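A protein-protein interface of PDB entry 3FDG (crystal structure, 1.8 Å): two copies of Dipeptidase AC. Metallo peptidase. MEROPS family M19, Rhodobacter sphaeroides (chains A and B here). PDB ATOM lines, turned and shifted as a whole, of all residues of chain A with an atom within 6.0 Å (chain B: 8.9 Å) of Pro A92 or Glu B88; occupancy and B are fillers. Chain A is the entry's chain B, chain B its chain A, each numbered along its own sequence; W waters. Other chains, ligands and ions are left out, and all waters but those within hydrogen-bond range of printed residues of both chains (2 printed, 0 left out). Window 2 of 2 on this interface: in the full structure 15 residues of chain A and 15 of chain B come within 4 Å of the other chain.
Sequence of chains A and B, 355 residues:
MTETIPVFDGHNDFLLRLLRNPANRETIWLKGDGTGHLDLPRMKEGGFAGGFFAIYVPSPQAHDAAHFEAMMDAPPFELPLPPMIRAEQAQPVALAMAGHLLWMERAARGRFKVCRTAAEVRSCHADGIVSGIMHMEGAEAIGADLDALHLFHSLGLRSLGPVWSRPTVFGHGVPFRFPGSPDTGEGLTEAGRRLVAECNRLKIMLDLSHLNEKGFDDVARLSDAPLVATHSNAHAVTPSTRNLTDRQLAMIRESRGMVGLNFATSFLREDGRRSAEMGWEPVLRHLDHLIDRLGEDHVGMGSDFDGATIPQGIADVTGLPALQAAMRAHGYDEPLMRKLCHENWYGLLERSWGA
Of the 18 printed residues of chain B, 5 touch a printed residue of chain A. Among the printed residues, 8 pairs touch across the chains. Among the printed residues, no Asp or Glu carboxylate lies within 4 Å of a Lys or Arg side-chain nitrogen of the other chain.
Water W2 bridges OE1 of Gln B91 (2.6 Å) and O of Pro A92 (2.7 Å). Water W1 bridges OE1 of Gln A91 (2.6 Å) and O of Pro B92 (2.7 Å).
Glu A88 touches Pro B92, and with the chains exchanged Pro A92 touches Glu B88. Gln A91 touches Pro B92, and with the chains exchanged Pro A92 touches Gln B91. Gln A91 touches Leu B95, and with the chains exchanged Leu A95 touches Gln B91. Leu A95 touches its own counterpart, Leu B95. Positions printed for both chains: 87, 88, 89, 90, 91, 92, 93, 94 and 95. Of the 8 pairs that touch across the chains among the printed residues, 7 have their exchanged pair printed and touching as well.
OE2 of Glu B88 is in hydrogen-bond range of NE2 of Gln B89 (3.2 Å). The side-chain amide nitrogen of Gln B91 is in hydrogen-bond range of the backbone carbonyl oxygen of Ala B141 (3.0 Å). The side-chain carboxylate (OE1) of Glu A88 lies within hydrogen-bond range of the side-chain amide nitrogen (NE2) of Gln A89 (3.3 Å).
Pro A92 touches just these residues of chain B: Glu B88 (3.5 Å) and Gln B91 (3.6 Å). Of the printed residues of chain A, Gln B91 touches Pro A92 (3.6 Å) and Leu A95 (3.7 Å). Of the printed residues of chain A, Leu B95 touches Gln A91 (3.8 Å) and Leu A95 (3.7 Å). Printed residues of chain B within 4 Å of Leu A95: Gln B91, Leu B95 and Leu B151. Printed residues of chain A within 4 Å of Pro B92: Glu A88 and Gln A91. Arg B86 touches none of the printed residues of chain A. The nearest residue of chain A that does not touch Glu B88 is Glu A88 (5.2 Å).
Pro B92 touches Glu A88 (CG to O, 3.5 Å). Gln A91 touches Pro B92. CD1 of Leu B95 touches OE1 of Gln A91 (3.8 Å). CG of Pro A92 touches O of Glu B88, 3.5 Å away. Pro A92 touches Gln B91 (CA to OE1, 3.6 Å). Leu A95 touches Gln B91 (CD1 to OE1, 3.7 Å). Leu A95 touches Leu B95. Leu A95 touches Leu B151 (O to CD1, 3.2 Å).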
ATOM      1  N   ALA A  87      35.359 -24.448 -28.961  1.00  0.00           N
ATOM      2  CA  ALA A  87      34.410 -25.554 -28.799  1.00  0.00           C
ATOM      3  C   ALA A  87      33.739 -25.610 -27.402  1.00  0.00           C
ATOM      4  O   ALA A  87      32.544 -25.868 -27.317  1.00  0.00           O
ATOM      5  CB  ALA A  87      35.098 -26.877 -29.104  1.00  0.00           C
ATOM      6  N   GLU A  88      34.495 -25.290 -26.336  1.00  0.00           N
ATOM      7  CA  GLU A  88      33.964 -25.338 -24.960  1.00  0.00           C
ATOM      8  C   GLU A  88      32.762 -24.411 -24.834  1.00  0.00           C
ATOM      9  O   GLU A  88      31.786 -24.797 -24.212  1.00  0.00           O
ATOM     10  CB  GLU A  88      35.029 -24.943 -23.891  1.00  0.00           C
ATOM     11  CG  GLU A  88      34.519 -25.227 -22.450  1.00  0.00           C
ATOM     12  CD  GLU A  88      35.506 -24.909 -21.333  1.00  0.00           C
ATOM     13  OE1 GLU A  88      36.036 -23.779 -21.269  1.00  0.00           O
ATOM     14  OE2 GLU A  88      35.734 -25.804 -20.494  1.00  0.00           O
ATOM     15  N   GLN A  89      32.840 -23.214 -25.441  1.00  0.00           N
ATOM     16  CA  GLN A  89      31.736 -22.252 -25.435  1.00  0.00           C
ATOM     17  C   GLN A  89      30.679 -22.552 -26.511  1.00  0.00           C
ATOM     18  O   GLN A  89      29.476 -22.303 -26.309  1.00  0.00           O
ATOM     19  CB  GLN A  89      32.266 -20.813 -25.597  1.00  0.00           C
ATOM     20  CG  GLN A  89      32.903 -20.230 -24.309  1.00  0.00           C
ATOM     21  CD  GLN A  89      34.111 -21.027 -23.914  1.00  0.00           C
ATOM     22  OE1 GLN A  89      35.060 -21.209 -24.701  1.00  0.00           O
ATOM     23  NE2 GLN A  89      34.067 -21.580 -22.721  1.00  0.00           N
ATOM     24  N   ALA A  90      31.101 -23.097 -27.649  1.00  0.00           N
ATOM     25  CA  ALA A  90      30.170 -23.265 -28.763  1.00  0.00           C
ATOM     26  C   ALA A  90      29.288 -24.491 -28.551  1.00  0.00           C
ATOM     27  O   ALA A  90      28.093 -24.503 -28.919  1.00  0.00           O
ATOM     28  CB  ALA A  90      30.972 -23.396 -30.095  1.00  0.00           C
ATOM     29  N   GLN A  91      29.876 -25.541 -27.983  1.00  0.00           N
ATOM     30  CA  GLN A  91      29.169 -26.816 -27.848  1.00  0.00           C
ATOM     31  C   GLN A  91      27.775 -26.773 -27.145  1.00  0.00           C
ATOM     32  O   GLN A  91      26.796 -27.255 -27.713  1.00  0.00           O
ATOM     33  CB  GLN A  91      30.105 -27.904 -27.291  1.00  0.00           C
ATOM     34  CG  GLN A  91      31.061 -28.444 -28.409  1.00  0.00           C
ATOM     35  CD  GLN A  91      32.058 -29.440 -27.864  1.00  0.00           C
ATOM     36  OE1 GLN A  91      32.190 -29.600 -26.638  1.00  0.00           O
ATOM     37  NE2 GLN A  91      32.763 -30.143 -28.770  1.00  0.00           N
ATOM     38  N   PRO A  92      27.657 -26.138 -25.960  1.00  0.00           N
ATOM     39  CA  PRO A  92      26.303 -26.062 -25.356  1.00  0.00           C
ATOM     40  C   PRO A  92      25.263 -25.403 -26.289  1.00  0.00           C
ATOM     41  O   PRO A  92      24.082 -25.805 -26.303  1.00  0.00           O
ATOM     42  CB  PRO A  92      26.526 -25.166 -24.101  1.00  0.00           C
ATOM     43  CG  PRO A  92      27.971 -25.419 -23.758  1.00  0.00           C
ATOM     44  CD  PRO A  92      28.682 -25.545 -25.089  1.00  0.00           C
ATOM     45  N   VAL A  93      25.689 -24.372 -27.027  1.00  0.00           N
ATOM     46  CA  VAL A  93      24.796 -23.634 -27.921  1.00  0.00           C
ATOM     47  C   VAL A  93      24.434 -24.514 -29.102  1.00  0.00           C
ATOM     48  O   VAL A  93      23.264 -24.602 -29.457  1.00  0.00           O
ATOM     49  CB  VAL A  93      25.409 -22.246 -28.382  1.00  0.00           C
ATOM     50  CG1 VAL A  93      24.454 -21.549 -29.406  1.00  0.00           C
ATOM     51  CG2 VAL A  93      25.694 -21.378 -27.147  1.00  0.00           C
ATOM     52  N   ALA A  94      25.410 -25.205 -29.686  1.00  0.00           N
ATOM     53  CA  ALA A  94      25.091 -26.087 -30.852  1.00  0.00           C
ATOM     54  C   ALA A  94      24.238 -27.253 -30.416  1.00  0.00           C
ATOM     55  O   ALA A  94      23.362 -27.681 -31.150  1.00  0.00           O
ATOM     56  CB  ALA A  94      26.331 -26.583 -31.523  1.00  0.00           C
ATOM     57  N   LEU A  95      24.477 -27.791 -29.215  1.00  0.00           N
ATOM     58  CA  LEU A  95      23.574 -28.827 -28.705  1.00  0.00           C
ATOM     59  C   LEU A  95      22.179 -28.333 -28.411  1.00  0.00           C
ATOM     60  O   LEU A  95      21.227 -29.053 -28.693  1.00  0.00           O
ATOM     61  CB  LEU A  95      24.123 -29.499 -27.456  1.00  0.00           C
ATOM     62  CG  LEU A  95      25.303 -30.441 -27.557  1.00  0.00           C
ATOM     63  CD1 LEU A  95      25.580 -30.921 -26.139  1.00  0.00           C
ATOM     64  CD2 LEU A  95      25.004 -31.645 -28.438  1.00  0.00           C
ATOM     65  N   ALA A  96      22.043 -27.134 -27.874  1.00  0.00           N
ATOM     66  CA  ALA A  96      20.714 -26.528 -27.713  1.00  0.00           C
ATOM     67  C   ALA A  96      19.944 -26.496 -29.034  1.00  0.00           C
ATOM     68  O   ALA A  96      18.779 -26.909 -29.095  1.00  0.00           O
ATOM     69  CB  ALA A  96      20.825 -25.131 -27.104  1.00  0.00           C
ATOM     70  N   MET A  97      20.578 -25.973 -30.080  1.00  0.00           N
ATOM     71  CA  MET A  97      19.945 -25.877 -31.410  1.00  0.00           C
ATOM     72  C   MET A  97      19.661 -27.224 -32.041  1.00  0.00           C
ATOM     73  O   MET A  97      18.552 -27.434 -32.527  1.00  0.00           O
ATOM     74  CB  MET A  97      20.785 -24.956 -32.332  1.00  0.00           C
ATOM     75  CG  MET A  97      20.818 -23.523 -31.724  1.00  0.00           C
ATOM     76  SD  MET A  97      21.915 -22.350 -32.642  1.00  0.00           S
ATOM     77  CE  MET A  97      20.837 -21.866 -33.838  1.00  0.00           C
ATOM     78  N   VAL B  57      31.004 -37.070 -15.486  1.00  0.00           N
ATOM     79  CA  VAL B  57      31.564 -35.720 -15.419  1.00  0.00           C
ATOM     80  C   VAL B  57      32.157 -35.527 -14.021  1.00  0.00           C
ATOM     81  O   VAL B  57      31.444 -35.539 -13.043  1.00  0.00           O
ATOM     82  CB  VAL B  57      30.518 -34.655 -15.745  1.00  0.00           C
ATOM     83  CG1 VAL B  57      31.089 -33.210 -15.578  1.00  0.00           C
ATOM     84  CG2 VAL B  57      30.008 -34.907 -17.162  1.00  0.00           C
ATOM     85  N   ILE B  85      26.744 -29.530 -10.828  1.00  0.00           N
ATOM     86  CA  ILE B  85      27.286 -29.017 -12.117  1.00  0.00           C
ATOM     87  C   ILE B  85      26.094 -28.922 -13.072  1.00  0.00           C
ATOM     88  O   ILE B  85      25.277 -29.881 -13.192  1.00  0.00           O
ATOM     89  CB  ILE B  85      28.408 -29.966 -12.692  1.00  0.00           C
ATOM     90  CG1 ILE B  85      29.588 -30.036 -11.714  1.00  0.00           C
ATOM     91  CG2 ILE B  85      28.924 -29.506 -14.084  1.00  0.00           C
ATOM     92  CD1 ILE B  85      30.500 -31.264 -11.891  1.00  0.00           C
ATOM     93  N   ARG B  86      25.940 -27.759 -13.722  1.00  0.00           N
ATOM     94  CA  ARG B  86      24.787 -27.590 -14.621  1.00  0.00           C
ATOM     95  C   ARG B  86      25.144 -27.997 -16.060  1.00  0.00           C
ATOM     96  O   ARG B  86      26.317 -28.164 -16.347  1.00  0.00           O
ATOM     97  CB  ARG B  86      24.212 -26.171 -14.546  1.00  0.00           C
ATOM     98  CG  ARG B  86      23.755 -25.778 -13.126  1.00  0.00           C
ATOM     99  CD  ARG B  86      22.656 -26.740 -12.615  1.00  0.00           C
ATOM    100  NE  ARG B  86      21.420 -26.529 -13.362  1.00  0.00           N
ATOM    101  CZ  ARG B  86      20.560 -25.543 -13.111  1.00  0.00           C
ATOM    102  NH1 ARG B  86      19.461 -25.424 -13.843  1.00  0.00           N
ATOM    103  NH2 ARG B  86      20.790 -24.686 -12.115  1.00  0.00           N
ATOM    104  N   ALA B  87      24.129 -28.171 -16.910  1.00  0.00           N
ATOM    105  CA  ALA B  87      24.284 -28.688 -18.293  1.00  0.00           C
ATOM    106  C   ALA B  87      25.309 -27.910 -19.126  1.00  0.00           C
ATOM    107  O   ALA B  87      26.162 -28.511 -19.788  1.00  0.00           O
ATOM    108  CB  ALA B  87      22.935 -28.780 -18.985  1.00  0.00           C
ATOM    109  N   GLU B  88      25.288 -26.579 -19.017  1.00  0.00           N
ATOM    110  CA  GLU B  88      26.300 -25.746 -19.705  1.00  0.00           C
ATOM    111  C   GLU B  88      27.751 -26.144 -19.431  1.00  0.00           C
ATOM    112  O   GLU B  88      28.572 -26.160 -20.375  1.00  0.00           O
ATOM    113  CB  GLU B  88      26.124 -24.262 -19.308  1.00  0.00           C
ATOM    114  CG  GLU B  88      26.849 -23.268 -20.268  1.00  0.00           C
ATOM    115  CD  GLU B  88      26.680 -21.810 -19.792  1.00  0.00           C
ATOM    116  OE1 GLU B  88      26.015 -21.035 -20.504  1.00  0.00           O
ATOM    117  OE2 GLU B  88      27.181 -21.453 -18.699  1.00  0.00           O
ATOM    118  N   GLN B  89      28.095 -26.445 -18.169  1.00  0.00           N
ATOM    119  CA  GLN B  89      29.449 -26.879 -17.871  1.00  0.00           C
ATOM    120  C   GLN B  89      29.634 -28.375 -18.105  1.00  0.00           C
ATOM    121  O   GLN B  89      30.752 -28.824 -18.372  1.00  0.00           O
ATOM    122  CB  GLN B  89      29.884 -26.577 -16.411  1.00  0.00           C
ATOM    123  CG  GLN B  89      30.280 -25.147 -16.125  1.00  0.00           C
ATOM    124  CD  GLN B  89      29.134 -24.215 -16.362  1.00  0.00           C
ATOM    125  OE1 GLN B  89      28.028 -24.442 -15.870  1.00  0.00           O
ATOM    126  NE2 GLN B  89      29.370 -23.169 -17.138  1.00  0.00           N
ATOM    127  N   ALA B  90      28.590 -29.167 -17.929  1.00  0.00           N
ATOM    128  CA  ALA B  90      28.786 -30.632 -18.067  1.00  0.00           C
ATOM    129  C   ALA B  90      28.844 -31.098 -19.513  1.00  0.00           C
ATOM    130  O   ALA B  90      29.549 -32.107 -19.848  1.00  0.00           O
ATOM    131  CB  ALA B  90      27.628 -31.378 -17.369  1.00  0.00           C
ATOM    132  N   GLN B  91      28.057 -30.443 -20.350  1.00  0.00           N
ATOM    133  CA  GLN B  91      27.922 -30.873 -21.746  1.00  0.00           C
ATOM    134  C   GLN B  91      29.238 -31.030 -22.535  1.00  0.00           C
ATOM    135  O   GLN B  91      29.444 -32.074 -23.128  1.00  0.00           O
ATOM    136  CB  GLN B  91      26.930 -30.029 -22.524  1.00  0.00           C
ATOM    137  CG  GLN B  91      25.513 -30.560 -22.273  1.00  0.00           C
ATOM    138  CD  GLN B  91      24.481 -29.688 -22.848  1.00  0.00           C
ATOM    139  OE1 GLN B  91      24.775 -28.614 -23.415  1.00  0.00           O
ATOM    140  NE2 GLN B  91      23.239 -30.133 -22.747  1.00  0.00           N
ATOM    141  N   PRO B  92      30.141 -30.018 -22.500  1.00  0.00           N
ATOM    142  CA  PRO B  92      31.411 -30.243 -23.193  1.00  0.00           C
ATOM    143  C   PRO B  92      32.219 -31.440 -22.671  1.00  0.00           C
ATOM    144  O   PRO B  92      32.903 -32.094 -23.475  1.00  0.00           O
ATOM    145  CB  PRO B  92      32.192 -28.928 -22.920  1.00  0.00           C
ATOM    146  CG  PRO B  92      31.106 -27.910 -22.664  1.00  0.00           C
ATOM    147  CD  PRO B  92      30.149 -28.714 -21.804  1.00  0.00           C
ATOM    148  N   VAL B  93      32.194 -31.694 -21.360  1.00  0.00           N
ATOM    149  CA  VAL B  93      32.904 -32.822 -20.786  1.00  0.00           C
ATOM    150  C   VAL B  93      32.250 -34.110 -21.239  1.00  0.00           C
ATOM    151  O   VAL B  93      32.953 -35.025 -21.700  1.00  0.00           O
ATOM    152  CB  VAL B  93      32.957 -32.806 -19.225  1.00  0.00           C
ATOM    153  CG1 VAL B  93      33.759 -34.049 -18.719  1.00  0.00           C
ATOM    154  CG2 VAL B  93      33.586 -31.456 -18.699  1.00  0.00           C
ATOM    155  N   ALA B  94      30.916 -34.198 -21.132  1.00  0.00           N
ATOM    156  CA  ALA B  94      30.234 -35.430 -21.608  1.00  0.00           C
ATOM    157  C   ALA B  94      30.442 -35.660 -23.101  1.00  0.00           C
ATOM    158  O   ALA B  94      30.652 -36.839 -23.541  1.00  0.00           O
ATOM    159  CB  ALA B  94      28.735 -35.441 -21.282  1.00  0.00           C
ATOM    160  N   LEU B  95      30.443 -34.580 -23.901  1.00  0.00           N
ATOM    161  CA  LEU B  95      30.764 -34.759 -25.348  1.00  0.00           C
ATOM    162  C   LEU B  95      32.174 -35.221 -25.598  1.00  0.00           C
ATOM    163  O   LEU B  95      32.438 -35.983 -26.548  1.00  0.00           O
ATOM    164  CB  LEU B  95      30.570 -33.496 -26.158  1.00  0.00           C
ATOM    165  CG  LEU B  95      29.096 -33.145 -26.378  1.00  0.00           C
ATOM    166  CD1 LEU B  95      29.083 -31.741 -27.013  1.00  0.00           C
ATOM    167  CD2 LEU B  95      28.331 -34.163 -27.296  1.00  0.00           C
ATOM    168  N   GLU B 140      23.954 -34.770 -15.416  1.00  0.00           N
ATOM    169  CA  GLU B 140      24.238 -33.329 -15.495  1.00  0.00           C
ATOM    170  C   GLU B 140      24.220 -32.804 -16.937  1.00  0.00           C
ATOM    171  O   GLU B 140      23.783 -31.681 -17.173  1.00  0.00           O
ATOM    172  CB  GLU B 140      25.603 -33.002 -14.849  1.00  0.00           C
ATOM    173  CG  GLU B 140      25.556 -33.075 -13.330  1.00  0.00           C
ATOM    174  CD  GLU B 140      25.866 -34.485 -12.799  1.00  0.00           C
ATOM    175  OE1 GLU B 140      26.029 -35.444 -13.610  1.00  0.00           O
ATOM    176  OE2 GLU B 140      25.984 -34.583 -11.572  1.00  0.00           O
ATOM    177  N   ALA B 141      24.676 -33.605 -17.903  1.00  0.00           N
ATOM    178  CA  ALA B 141      24.699 -33.072 -19.277  1.00  0.00           C
ATOM    179  C   ALA B 141      23.298 -32.981 -19.910  1.00  0.00           C
ATOM    180  O   ALA B 141      23.146 -32.543 -21.045  1.00  0.00           O
ATOM    181  CB  ALA B 141      25.687 -33.889 -20.157  1.00  0.00           C
ATOM    182  N   ILE B 142      22.269 -33.447 -19.195  1.00  0.00           N
ATOM    183  CA  ILE B 142      20.924 -33.329 -19.717  1.00  0.00           C
ATOM    184  C   ILE B 142      20.230 -32.187 -18.947  1.00  0.00           C
ATOM    185  O   ILE B 142      20.178 -32.202 -17.704  1.00  0.00           O
ATOM    186  CB  ILE B 142      20.207 -34.688 -19.600  1.00  0.00           C
ATOM    187  CG1 ILE B 142      20.984 -35.725 -20.442  1.00  0.00           C
ATOM    188  CG2 ILE B 142      18.728 -34.623 -20.045  1.00  0.00           C
ATOM    189  CD1 ILE B 142      20.623 -37.091 -20.059  1.00  0.00           C
ATOM    190  N   GLY B 143      19.695 -31.207 -19.685  1.00  0.00           N
ATOM    191  CA  GLY B 143      18.924 -30.146 -19.055  1.00  0.00           C
ATOM    192  C   GLY B 143      17.593 -30.628 -18.504  1.00  0.00           C
ATOM    193  O   GLY B 143      17.102 -31.655 -18.897  1.00  0.00           O
ATOM    194  N   ALA B 148      18.423 -32.692 -24.521  1.00  0.00           N
ATOM    195  CA  ALA B 148      19.695 -33.440 -24.664  1.00  0.00           C
ATOM    196  C   ALA B 148      19.597 -34.950 -24.519  1.00  0.00           C
ATOM    197  O   ALA B 148      20.437 -35.683 -25.084  1.00  0.00           O
ATOM    198  CB  ALA B 148      20.779 -32.871 -23.723  1.00  0.00           C
ATOM    199  N   LEU B 151      19.076 -36.206 -27.911  1.00  0.00           N
ATOM    200  CA  LEU B 151      20.363 -36.108 -28.652  1.00  0.00           C
ATOM    201  C   LEU B 151      21.354 -37.198 -28.291  1.00  0.00           C
ATOM    202  O   LEU B 151      21.955 -37.868 -29.177  1.00  0.00           O
ATOM    203  CB  LEU B 151      21.042 -34.741 -28.365  1.00  0.00           C
ATOM    204  CG  LEU B 151      20.314 -33.527 -28.920  1.00  0.00           C
ATOM    205  CD1 LEU B 151      21.089 -32.280 -28.491  1.00  0.00           C
ATOM    206  CD2 LEU B 151      20.285 -33.664 -30.503  1.00  0.00           C
HETATM  207  O   HOH W   1      34.196 -30.862 -25.456  1.00  0.00           O
HETATM  208  O   HOH W   2      23.118 -26.723 -23.991  1.00  0.00           O
